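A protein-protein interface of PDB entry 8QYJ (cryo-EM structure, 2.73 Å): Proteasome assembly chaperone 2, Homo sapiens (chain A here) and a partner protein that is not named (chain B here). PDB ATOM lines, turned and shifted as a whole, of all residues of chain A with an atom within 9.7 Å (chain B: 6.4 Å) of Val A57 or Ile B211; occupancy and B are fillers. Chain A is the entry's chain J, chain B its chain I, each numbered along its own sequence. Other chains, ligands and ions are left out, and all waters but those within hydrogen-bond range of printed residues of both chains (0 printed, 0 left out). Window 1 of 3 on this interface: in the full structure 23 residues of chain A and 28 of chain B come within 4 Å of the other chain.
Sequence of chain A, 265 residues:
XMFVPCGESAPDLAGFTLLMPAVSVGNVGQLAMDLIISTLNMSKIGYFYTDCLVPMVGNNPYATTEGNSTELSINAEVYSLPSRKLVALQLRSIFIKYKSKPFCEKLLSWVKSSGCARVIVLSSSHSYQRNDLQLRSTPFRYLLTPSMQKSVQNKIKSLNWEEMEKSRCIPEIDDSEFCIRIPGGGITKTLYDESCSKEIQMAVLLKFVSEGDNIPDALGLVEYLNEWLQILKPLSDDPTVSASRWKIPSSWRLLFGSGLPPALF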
ATOM      1  N   TYR A  47      26.697  20.216  16.574  1.00  0.00           N
ATOM      2  CA  TYR A  47      27.562  19.667  17.608  1.00  0.00           C
ATOM      3  C   TYR A  47      29.015  19.961  17.264  1.00  0.00           C
ATOM      4  O   TYR A  47      29.367  20.189  16.105  1.00  0.00           O
ATOM      5  CB  TYR A  47      27.382  18.146  17.768  1.00  0.00           C
ATOM      6  CG  TYR A  47      25.956  17.656  17.654  1.00  0.00           C
ATOM      7  CD1 TYR A  47      25.137  17.579  18.771  1.00  0.00           C
ATOM      8  CD2 TYR A  47      25.436  17.254  16.432  1.00  0.00           C
ATOM      9  CE1 TYR A  47      23.838  17.128  18.672  1.00  0.00           C
ATOM     10  CE2 TYR A  47      24.138  16.802  16.324  1.00  0.00           C
ATOM     11  CZ  TYR A  47      23.343  16.740  17.447  1.00  0.00           C
ATOM     12  OH  TYR A  47      22.048  16.290  17.343  1.00  0.00           O
ATOM     13  N   VAL A  54      35.531  13.595  28.033  1.00  0.00           N
ATOM     14  CA  VAL A  54      34.937  12.315  28.437  1.00  0.00           C
ATOM     15  C   VAL A  54      33.496  12.254  27.942  1.00  0.00           C
ATOM     16  O   VAL A  54      32.732  13.211  28.154  1.00  0.00           O
ATOM     17  CB  VAL A  54      35.004  12.156  29.958  1.00  0.00           C
ATOM     18  CG1 VAL A  54      34.419  10.820  30.382  1.00  0.00           C
ATOM     19  CG2 VAL A  54      36.438  12.292  30.439  1.00  0.00           C
ATOM     20  N   PRO A  55      33.081  11.177  27.277  1.00  0.00           N
ATOM     21  CA  PRO A  55      31.717  11.123  26.739  1.00  0.00           C
ATOM     22  C   PRO A  55      30.661  11.080  27.834  1.00  0.00           C
ATOM     23  O   PRO A  55      30.864  10.512  28.910  1.00  0.00           O
ATOM     24  CB  PRO A  55      31.709   9.829  25.915  1.00  0.00           C
ATOM     25  CG  PRO A  55      33.147   9.479  25.710  1.00  0.00           C
ATOM     26  CD  PRO A  55      33.866   9.987  26.912  1.00  0.00           C
ATOM     27  N   MET A  56      29.518  11.694  27.538  1.00  0.00           N
ATOM     28  CA  MET A  56      28.352  11.657  28.409  1.00  0.00           C
ATOM     29  C   MET A  56      27.123  11.943  27.559  1.00  0.00           C
ATOM     30  O   MET A  56      27.228  12.471  26.450  1.00  0.00           O
ATOM     31  CB  MET A  56      28.482  12.646  29.577  1.00  0.00           C
ATOM     32  CG  MET A  56      28.610  14.120  29.198  1.00  0.00           C
ATOM     33  SD  MET A  56      27.068  14.950  28.761  1.00  0.00           S
ATOM     34  CE  MET A  56      26.268  15.040  30.360  1.00  0.00           C
ATOM     35  N   VAL A  57      25.955  11.582  28.088  1.00  0.00           N
ATOM     36  CA  VAL A  57      24.715  11.677  27.327  1.00  0.00           C
ATOM     37  C   VAL A  57      23.552  11.850  28.296  1.00  0.00           C
ATOM     38  O   VAL A  57      23.598  11.391  29.440  1.00  0.00           O
ATOM     39  CB  VAL A  57      24.529  10.436  26.418  1.00  0.00           C
ATOM     40  CG1 VAL A  57      24.335   9.177  27.250  1.00  0.00           C
ATOM     41  CG2 VAL A  57      23.394  10.637  25.439  1.00  0.00           C
ATOM     42  N   GLY A  58      22.510  12.533  27.831  1.00  0.00           N
ATOM     43  CA  GLY A  58      21.318  12.756  28.629  1.00  0.00           C
ATOM     44  C   GLY A  58      20.240  13.396  27.781  1.00  0.00           C
ATOM     45  O   GLY A  58      20.424  13.645  26.587  1.00  0.00           O
ATOM     46  N   ASN A  59      19.101  13.661  28.416  1.00  0.00           N
ATOM     47  CA  ASN A  59      17.972  14.279  27.735  1.00  0.00           C
ATOM     48  C   ASN A  59      18.109  15.802  27.760  1.00  0.00           C
ATOM     49  O   ASN A  59      19.140  16.352  28.152  1.00  0.00           O
ATOM     50  CB  ASN A  59      16.653  13.821  28.354  1.00  0.00           C
ATOM     51  CG  ASN A  59      16.284  12.405  27.962  1.00  0.00           C
ATOM     52  OD1 ASN A  59      16.443  12.006  26.810  1.00  0.00           O
ATOM     53  ND2 ASN A  59      15.776  11.639  28.920  1.00  0.00           N
ATOM     54  N   ASN A  60      17.056  16.493  27.341  1.00  0.00           N
ATOM     55  CA  ASN A  60      17.104  17.940  27.148  1.00  0.00           C
ATOM     56  C   ASN A  60      17.244  18.664  28.481  1.00  0.00           C
ATOM     57  O   ASN A  60      16.380  18.508  29.354  1.00  0.00           O
ATOM     58  CB  ASN A  60      15.839  18.397  26.426  1.00  0.00           C
ATOM     59  CG  ASN A  60      15.941  19.814  25.904  1.00  0.00           C
ATOM     60  OD1 ASN A  60      16.975  20.466  26.035  1.00  0.00           O
ATOM     61  ND2 ASN A  60      14.862  20.298  25.303  1.00  0.00           N
ATOM     62  N   PRO A  61      18.294  19.464  28.683  1.00  0.00           N
ATOM     63  CA  PRO A  61      18.431  20.207  29.943  1.00  0.00           C
ATOM     64  C   PRO A  61      17.546  21.436  30.042  1.00  0.00           C
ATOM     65  O   PRO A  61      17.332  21.931  31.157  1.00  0.00           O
ATOM     66  CB  PRO A  61      19.917  20.609  29.954  1.00  0.00           C
ATOM     67  CG  PRO A  61      20.560  19.844  28.828  1.00  0.00           C
ATOM     68  CD  PRO A  61      19.483  19.614  27.831  1.00  0.00           C
ATOM     69  N   GLU A  71      14.543  14.992  24.014  1.00  0.00           N
ATOM     70  CA  GLU A  71      15.569  15.208  23.003  1.00  0.00           C
ATOM     71  C   GLU A  71      16.937  14.909  23.602  1.00  0.00           C
ATOM     72  O   GLU A  71      17.275  15.419  24.674  1.00  0.00           O
ATOM     73  CB  GLU A  71      15.521  16.641  22.471  1.00  0.00           C
ATOM     74  CG  GLU A  71      14.265  16.959  21.679  1.00  0.00           C
ATOM     75  CD  GLU A  71      14.235  18.389  21.180  1.00  0.00           C
ATOM     76  OE1 GLU A  71      15.132  19.171  21.557  1.00  0.00           O
ATOM     77  OE2 GLU A  71      13.312  18.732  20.412  1.00  0.00           O
ATOM     78  N   LEU A  72      17.715  14.086  22.905  1.00  0.00           N
ATOM     79  CA  LEU A  72      19.010  13.655  23.413  1.00  0.00           C
ATOM     80  C   LEU A  72      20.039  14.777  23.310  1.00  0.00           C
ATOM     81  O   LEU A  72      20.001  15.604  22.395  1.00  0.00           O
ATOM     82  CB  LEU A  72      19.494  12.428  22.646  1.00  0.00           C
ATOM     83  CG  LEU A  72      20.527  11.549  23.349  1.00  0.00           C
ATOM     84  CD1 LEU A  72      19.910  10.900  24.575  1.00  0.00           C
ATOM     85  CD2 LEU A  72      21.075  10.500  22.400  1.00  0.00           C
ATOM     86  N   SER A  73      20.970  14.794  24.261  1.00  0.00           N
ATOM     87  CA  SER A  73      22.026  15.795  24.305  1.00  0.00           C
ATOM     88  C   SER A  73      23.368  15.123  24.557  1.00  0.00           C
ATOM     89  O   SER A  73      23.441  14.054  25.168  1.00  0.00           O
ATOM     90  CB  SER A  73      21.758  16.844  25.392  1.00  0.00           C
ATOM     91  OG  SER A  73      21.822  16.267  26.684  1.00  0.00           O
ATOM     92  N   ILE A  74      24.435  15.765  24.078  1.00  0.00           N
ATOM     93  CA  ILE A  74      25.792  15.249  24.232  1.00  0.00           C
ATOM     94  C   ILE A  74      26.649  16.282  24.955  1.00  0.00           C
ATOM     95  O   ILE A  74      26.153  17.335  25.369  1.00  0.00           O
ATOM     96  CB  ILE A  74      26.406  14.863  22.874  1.00  0.00           C
ATOM     97  CG1 ILE A  74      26.725  16.107  22.046  1.00  0.00           C
ATOM     98  CG2 ILE A  74      25.477  13.930  22.111  1.00  0.00           C
ATOM     99  CD1 ILE A  74      27.893  15.923  21.104  1.00  0.00           C
ATOM    100  N   ASN A  75      27.940  15.987  25.114  1.00  0.00           N
ATOM    101  CA  ASN A  75      28.816  16.774  25.975  1.00  0.00           C
ATOM    102  C   ASN A  75      29.304  18.075  25.347  1.00  0.00           C
ATOM    103  O   ASN A  75      29.969  18.856  26.035  1.00  0.00           O
ATOM    104  CB  ASN A  75      30.024  15.933  26.399  1.00  0.00           C
ATOM    105  CG  ASN A  75      30.828  15.428  25.220  1.00  0.00           C
ATOM    106  OD1 ASN A  75      30.404  15.536  24.071  1.00  0.00           O
ATOM    107  ND2 ASN A  75      31.997  14.866  25.501  1.00  0.00           N
ATOM    108  N   ALA A  76      29.004  18.333  24.075  1.00  0.00           N
ATOM    109  CA  ALA A  76      29.446  19.568  23.428  1.00  0.00           C
ATOM    110  C   ALA A  76      28.442  19.921  22.340  1.00  0.00           C
ATOM    111  O   ALA A  76      28.328  19.200  21.346  1.00  0.00           O
ATOM    112  CB  ALA A  76      30.850  19.418  22.851  1.00  0.00           C
ATOM    113  N   GLU A  77      27.728  21.030  22.522  1.00  0.00           N
ATOM    114  CA  GLU A  77      26.654  21.415  21.620  1.00  0.00           C
ATOM    115  C   GLU A  77      26.736  22.911  21.347  1.00  0.00           C
ATOM    116  O   GLU A  77      27.311  23.674  22.126  1.00  0.00           O
ATOM    117  CB  GLU A  77      25.287  21.044  22.205  1.00  0.00           C
ATOM    118  CG  GLU A  77      25.032  19.548  22.224  1.00  0.00           C
ATOM    119  CD  GLU A  77      23.730  19.187  22.903  1.00  0.00           C
ATOM    120  OE1 GLU A  77      22.701  19.088  22.207  1.00  0.00           O
ATOM    121  OE2 GLU A  77      23.738  19.008  24.138  1.00  0.00           O
ATOM    122  N   ARG A  92      29.780  20.051  28.802  1.00  0.00           N
ATOM    123  CA  ARG A  92      29.187  19.415  29.973  1.00  0.00           C
ATOM    124  C   ARG A  92      30.032  18.256  30.489  1.00  0.00           C
ATOM    125  O   ARG A  92      29.504  17.321  31.092  1.00  0.00           O
ATOM    126  CB  ARG A  92      27.772  18.927  29.662  1.00  0.00           C
ATOM    127  CG  ARG A  92      26.890  19.940  28.962  1.00  0.00           C
ATOM    128  CD  ARG A  92      25.442  19.484  28.959  1.00  0.00           C
ATOM    129  NE  ARG A  92      24.552  20.487  28.390  1.00  0.00           N
ATOM    130  CZ  ARG A  92      24.297  20.613  27.095  1.00  0.00           C
ATOM    131  NH1 ARG A  92      24.847  19.808  26.201  1.00  0.00           N
ATOM    132  NH2 ARG A  92      23.468  21.568  26.687  1.00  0.00           N
ATOM    133  N   SER A  93      31.342  18.298  30.271  1.00  0.00           N
ATOM    134  CA  SER A  93      32.202  17.185  30.656  1.00  0.00           C
ATOM    135  C   SER A  93      33.568  17.732  31.054  1.00  0.00           C
ATOM    136  O   SER A  93      33.733  18.932  31.289  1.00  0.00           O
ATOM    137  CB  SER A  93      32.293  16.161  29.519  1.00  0.00           C
ATOM    138  OG  SER A  93      33.024  15.019  29.924  1.00  0.00           O
ATOM    139  N   ILE A  94      34.554  16.838  31.131  1.00  0.00           N
ATOM    140  CA  ILE A  94      35.903  17.173  31.564  1.00  0.00           C
ATOM    141  C   ILE A  94      36.900  16.644  30.543  1.00  0.00           C
ATOM    142  O   ILE A  94      36.596  15.762  29.737  1.00  0.00           O
ATOM    143  CB  ILE A  94      36.212  16.613  32.968  1.00  0.00           C
ATOM    144  CG1 ILE A  94      35.759  15.158  33.066  1.00  0.00           C
ATOM    145  CG2 ILE A  94      35.538  17.452  34.037  1.00  0.00           C
ATOM    146  CD1 ILE A  94      35.982  14.541  34.419  1.00  0.00           C
ATOM    147  N   SER A 251      16.576  21.677  34.907  1.00  0.00           N
ATOM    148  CA  SER A 251      17.461  20.610  35.357  1.00  0.00           C
ATOM    149  C   SER A 251      18.181  20.942  36.657  1.00  0.00           C
ATOM    150  O   SER A 251      18.948  20.108  37.150  1.00  0.00           O
ATOM    151  CB  SER A 251      18.485  20.285  34.267  1.00  0.00           C
ATOM    152  OG  SER A 251      19.105  21.461  33.779  1.00  0.00           O
ATOM    153  N   ASP B 174      23.293   5.227  42.025  1.00  0.00           N
ATOM    154  CA  ASP B 174      23.573   6.272  41.049  1.00  0.00           C
ATOM    155  C   ASP B 174      22.320   7.012  40.602  1.00  0.00           C
ATOM    156  O   ASP B 174      22.438   8.053  39.947  1.00  0.00           O
ATOM    157  CB  ASP B 174      24.276   5.673  39.829  1.00  0.00           C
ATOM    158  CG  ASP B 174      25.650   5.128  40.160  1.00  0.00           C
ATOM    159  OD1 ASP B 174      26.090   5.282  41.316  1.00  0.00           O
ATOM    160  OD2 ASP B 174      26.290   4.544  39.260  1.00  0.00           O
ATOM    161  N   LEU B 192      17.213   5.367  26.635  1.00  0.00           N
ATOM    162  CA  LEU B 192      17.521   6.597  25.920  1.00  0.00           C
ATOM    163  C   LEU B 192      17.622   6.287  24.433  1.00  0.00           C
ATOM    164  O   LEU B 192      18.101   5.220  24.041  1.00  0.00           O
ATOM    165  CB  LEU B 192      18.832   7.233  26.408  1.00  0.00           C
ATOM    166  CG  LEU B 192      18.851   7.876  27.796  1.00  0.00           C
ATOM    167  CD1 LEU B 192      20.279   8.144  28.239  1.00  0.00           C
ATOM    168  CD2 LEU B 192      18.043   9.161  27.806  1.00  0.00           C
ATOM    169  N   LEU B 206      14.606   7.782  30.672  1.00  0.00           N
ATOM    170  CA  LEU B 206      15.338   8.216  31.853  1.00  0.00           C
ATOM    171  C   LEU B 206      14.986   9.657  32.205  1.00  0.00           C
ATOM    172  O   LEU B 206      14.919  10.529  31.334  1.00  0.00           O
ATOM    173  CB  LEU B 206      16.842   8.080  31.619  1.00  0.00           C
ATOM    174  CG  LEU B 206      17.763   8.415  32.792  1.00  0.00           C
ATOM    175  CD1 LEU B 206      17.433   7.559  33.999  1.00  0.00           C
ATOM    176  CD2 LEU B 206      19.216   8.240  32.391  1.00  0.00           C
ATOM    177  N   GLU B 207      14.764   9.903  33.494  1.00  0.00           N
ATOM    178  CA  GLU B 207      14.383  11.228  33.954  1.00  0.00           C
ATOM    179  C   GLU B 207      15.534  12.213  33.754  1.00  0.00           C
ATOM    180  O   GLU B 207      16.666  11.839  33.442  1.00  0.00           O
ATOM    181  CB  GLU B 207      13.949  11.182  35.417  1.00  0.00           C
ATOM    182  CG  GLU B 207      12.523  10.694  35.609  1.00  0.00           C
ATOM    183  CD  GLU B 207      12.415   9.183  35.557  1.00  0.00           C
ATOM    184  OE1 GLU B 207      13.460   8.509  35.663  1.00  0.00           O
ATOM    185  OE2 GLU B 207      11.287   8.670  35.403  1.00  0.00           O
ATOM    186  N   GLN B 208      15.224  13.503  33.945  1.00  0.00           N
ATOM    187  CA  GLN B 208      16.128  14.546  33.457  1.00  0.00           C
ATOM    188  C   GLN B 208      17.453  14.574  34.210  1.00  0.00           C
ATOM    189  O   GLN B 208      18.495  14.276  33.598  1.00  0.00           O
ATOM    190  CB  GLN B 208      15.417  15.899  33.471  1.00  0.00           C
ATOM    191  CG  GLN B 208      14.297  16.010  32.445  1.00  0.00           C
ATOM    192  CD  GLN B 208      14.785  15.854  31.020  1.00  0.00           C
ATOM    193  OE1 GLN B 208      15.948  16.108  30.719  1.00  0.00           O
ATOM    194  NE2 GLN B 208      13.894  15.430  30.133  1.00  0.00           N
ATOM    195  N   PRO B 209      17.503  14.877  35.526  1.00  0.00           N
ATOM    196  CA  PRO B 209      18.803  15.175  36.153  1.00  0.00           C
ATOM    197  C   PRO B 209      19.786  14.010  36.147  1.00  0.00           C
ATOM    198  O   PRO B 209      20.902  14.135  36.661  1.00  0.00           O
ATOM    199  CB  PRO B 209      18.418  15.564  37.586  1.00  0.00           C
ATOM    200  CG  PRO B 209      17.147  14.857  37.830  1.00  0.00           C
ATOM    201  CD  PRO B 209      16.416  14.846  36.522  1.00  0.00           C
ATOM    202  N   ASN B 210      19.390  12.880  35.569  1.00  0.00           N
ATOM    203  CA  ASN B 210      20.244  11.705  35.486  1.00  0.00           C
ATOM    204  C   ASN B 210      20.960  11.665  34.142  1.00  0.00           C
ATOM    205  O   ASN B 210      20.367  11.954  33.100  1.00  0.00           O
ATOM    206  CB  ASN B 210      19.421  10.432  35.681  1.00  0.00           C
ATOM    207  CG  ASN B 210      18.863  10.311  37.083  1.00  0.00           C
ATOM    208  OD1 ASN B 210      19.592  10.019  38.030  1.00  0.00           O
ATOM    209  ND2 ASN B 210      17.564  10.537  37.223  1.00  0.00           N
ATOM    210  N   ILE B 211      22.244  11.306  34.176  1.00  0.00           N
ATOM    211  CA  ILE B 211      23.078  11.232  32.984  1.00  0.00           C
ATOM    212  C   ILE B 211      23.849   9.918  32.994  1.00  0.00           C
ATOM    213  O   ILE B 211      23.994   9.261  34.027  1.00  0.00           O
ATOM    214  CB  ILE B 211      24.055  12.423  32.876  1.00  0.00           C
ATOM    215  CG1 ILE B 211      24.915  12.522  34.137  1.00  0.00           C
ATOM    216  CG2 ILE B 211      23.299  13.720  32.632  1.00  0.00           C
ATOM    217  CD1 ILE B 211      26.255  13.172  33.911  1.00  0.00           C
ATOM    218  N   VAL B 212      24.343   9.540  31.817  1.00  0.00           N
ATOM    219  CA  VAL B 212      25.111   8.315  31.626  1.00  0.00           C
ATOM    220  C   VAL B 212      26.431   8.671  30.957  1.00  0.00           C
ATOM    221  O   VAL B 212      26.472   9.528  30.069  1.00  0.00           O
ATOM    222  CB  VAL B 212      24.338   7.281  30.777  1.00  0.00           C
ATOM    223  CG1 VAL B 212      25.028   5.928  30.821  1.00  0.00           C
ATOM    224  CG2 VAL B 212      22.901   7.165  31.250  1.00  0.00           C
ATOM    225  N   HIS B 213      27.511   8.017  31.386  1.00  0.00           N
ATOM    226  CA  HIS B 213      28.816   8.248  30.776  1.00  0.00           C
ATOM    227  C   HIS B 213      29.497   6.936  30.403  1.00  0.00           C
ATOM    228  O   HIS B 213      28.865   5.875  30.433  1.00  0.00           O
ATOM    229  CB  HIS B 213      29.704   9.080  31.707  1.00  0.00           C
ATOM    230  CG  HIS B 213      30.045   8.401  32.997  1.00  0.00           C
ATOM    231  ND1 HIS B 213      31.169   7.619  33.152  1.00  0.00           N
ATOM    232  CD2 HIS B 213      29.418   8.399  34.196  1.00  0.00           C
ATOM    233  CE1 HIS B 213      31.215   7.159  34.389  1.00  0.00           C
ATOM    234  NE2 HIS B 213      30.164   7.618  35.043  1.00  0.00           N
ATOM    235  N   PRO B 216      28.934   3.125  26.807  1.00  0.00           N
ATOM    236  CA  PRO B 216      27.600   3.252  26.194  1.00  0.00           C
ATOM    237  C   PRO B 216      27.280   4.672  25.771  1.00  0.00           C
ATOM    238  O   PRO B 216      26.673   4.887  24.711  1.00  0.00           O
ATOM    239  CB  PRO B 216      26.657   2.759  27.300  1.00  0.00           C
ATOM    240  CG  PRO B 216      27.499   1.916  28.178  1.00  0.00           C
ATOM    241  CD  PRO B 216      28.857   2.528  28.153  1.00  0.00           C
ATOM    242  N   ALA B 217      27.693   5.655  26.573  1.00  0.00           N
ATOM    243  CA  ALA B 217      27.518   7.050  26.189  1.00  0.00           C
ATOM    244  C   ALA B 217      28.314   7.376  24.935  1.00  0.00           C
ATOM    245  O   ALA B 217      27.848   8.131  24.078  1.00  0.00           O
ATOM    246  CB  ALA B 217      27.926   7.969  27.337  1.00  0.00           C
ATOM    247  N   ALA B 218      29.521   6.820  24.812  1.00  0.00           N
ATOM    248  CA  ALA B 218      30.328   7.055  23.621  1.00  0.00           C
ATOM    249  C   ALA B 218      29.637   6.518  22.373  1.00  0.00           C
ATOM    250  O   ALA B 218      29.571   7.198  21.342  1.00  0.00           O
ATOM    251  CB  ALA B 218      31.708   6.422  23.790  1.00  0.00           C
ATOM    252  N   LEU B 220      26.383   5.879  21.956  1.00  0.00           N
ATOM    253  CA  LEU B 220      25.166   6.639  21.690  1.00  0.00           C
ATOM    254  C   LEU B 220      25.485   8.008  21.101  1.00  0.00           C
ATOM    255  O   LEU B 220      24.784   8.482  20.202  1.00  0.00           O
ATOM    256  CB  LEU B 220      24.341   6.778  22.969  1.00  0.00           C
ATOM    257  CG  LEU B 220      22.836   6.974  22.778  1.00  0.00           C
ATOM    258  CD1 LEU B 220      22.245   5.847  21.948  1.00  0.00           C
ATOM    259  CD2 LEU B 220      22.134   7.077  24.118  1.00  0.00           C
ATOM    260  N   SER B 221      26.542   8.659  21.596  1.00  0.00           N
ATOM    261  CA  SER B 221      26.947   9.950  21.052  1.00  0.00           C
ATOM    262  C   SER B 221      27.405   9.822  19.608  1.00  0.00           C
ATOM    263  O   SER B 221      27.072  10.667  18.768  1.00  0.00           O
ATOM    264  CB  SER B 221      28.056  10.554  21.912  1.00  0.00           C
ATOM    265  OG  SER B 221      27.640  10.691  23.259  1.00  0.00           O
ATOM    266  N   LEU B 232      19.486   2.675  23.862  1.00  0.00           N
ATOM    267  CA  LEU B 232      20.271   2.205  24.995  1.00  0.00           C
ATOM    268  C   LEU B 232      19.332   1.824  26.129  1.00  0.00           C
ATOM    269  O   LEU B 232      18.422   2.586  26.467  1.00  0.00           O
ATOM    270  CB  LEU B 232      21.263   3.277  25.454  1.00  0.00           C
ATOM    271  CG  LEU B 232      21.851   3.151  26.859  1.00  0.00           C
ATOM    272  CD1 LEU B 232      22.815   1.983  26.939  1.00  0.00           C
ATOM    273  CD2 LEU B 232      22.543   4.442  27.257  1.00  0.00           C
ATOM    274  N   TYR B 236      18.872  -0.469  36.508  1.00  0.00           N
ATOM    275  CA  TYR B 236      19.329   0.002  37.811  1.00  0.00           C
ATOM    276  C   TYR B 236      19.003  -1.068  38.845  1.00  0.00           C
ATOM    277  O   TYR B 236      17.832  -1.304  39.155  1.00  0.00           O
ATOM    278  CB  TYR B 236      18.673   1.333  38.165  1.00  0.00           C
ATOM    279  CG  TYR B 236      19.258   2.516  37.432  1.00  0.00           C
ATOM    280  CD1 TYR B 236      20.399   3.152  37.899  1.00  0.00           C
ATOM    281  CD2 TYR B 236      18.671   2.996  36.269  1.00  0.00           C
ATOM    282  CE1 TYR B 236      20.938   4.231  37.232  1.00  0.00           C
ATOM    283  CE2 TYR B 236      19.202   4.076  35.596  1.00  0.00           C
ATOM    284  CZ  TYR B 236      20.335   4.690  36.081  1.00  0.00           C
ATOM    285  OH  TYR B 236      20.870   5.768  35.414  1.00  0.00           O
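The backbone carbonyl oxygen (O) of Glu A71 sits at hydrogen-bond distance from the backbone NH (N) of Asn A60. The backbone carbonyl oxygen (O) of Asn A59 sits at hydrogen-bond distance from the side-chain hydroxyl (OG) of Ser A73 (3.1 Å). The backbone NH (N) of Leu B232 sits at hydrogen-bond distance from the backbone carbonyl oxygen (O) of Leu B192 (2.9 Å). The side-chain hydroxyl (OG) of Ser B221 lies within hydrogen-bond range of the backbone carbonyl oxygen (O) of Ala B217 (2.7 Å).
Of the 20 printed residues of chain A, 6 touch a printed residue of chain B. Hydrophobic or aromatic side chains of chain A within 4 Å of the printed part of chain B: Pro A55, Met A56, Val A57 and Leu A72.
His B213 touches Pro A55. Pro A55 touches Ala B218. CG2 of Ile B211 touches CE of Met A56, at 3.96 Å. CA of Met A56 touches O of Val B212, 3.3 Å away. Met A56 touches Ala B217. Met A56 touches Ser B221 (O to OG, 3.7 Å). Val A57 touches Ile B211 (O to CA, 3.6 Å). Val A57 touches Ala B217. OD1 of Asn A59 touches CD2 of Leu B192, at 3.4 Å. Asn A59 touches Gln B208 (CB to OE1, 3.4 Å).
O of Val B212 is in hydrogen-bond range of N of Val A57 (2.9 Å). ND2 of Asn A59 is in hydrogen-bond range of O of Leu B206 (2.8 Å). The side-chain amide oxygen of Gln B208 sits close to the backbone carbonyl oxygen of Asn A60.
Printed residues of chain B within 4 Å of Val A57: Ile B211 (3.6 Å), Val B212 (2.9 Å) and Ala B217 (3.8 Å). Ile B211 touches just these residues of chain A: Met A56 (3.96 Å) and Val A57 (3.6 Å). No residue of chain A comes within 4 Å of Asn B210. Of chain A, only Met A56 (3.9 Å) and Val A57 (3.8 Å) come within 4 Å of Ala B217. Printed residues of chain A within 4 Å of Leu B192: Asn A59. Of the printed residues of chain B, Met A56 touches Ile B211, Val B212, Ala B217 and Ser B221. Printed residues of chain B within 4 Å of Leu A72: Leu B220 (3.96 Å). Printed residues of chain A within 4 Å of Ala B218: Pro A55. Of the printed residues of chain B, Asn A59 touches Leu B192, Leu B206 and Gln B208. Ser A73 touches none of the printed residues of chain B. The nearest printed residue of chain B that does not touch Val A57 is Leu B220 (4.001 Å). The nearest residue of chain A that does not touch Ile B211 is Gly A58 (4.6 Å). The nearest printed residue of chain A that does not touch Leu B192 is Leu A72 (4.1 Å).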
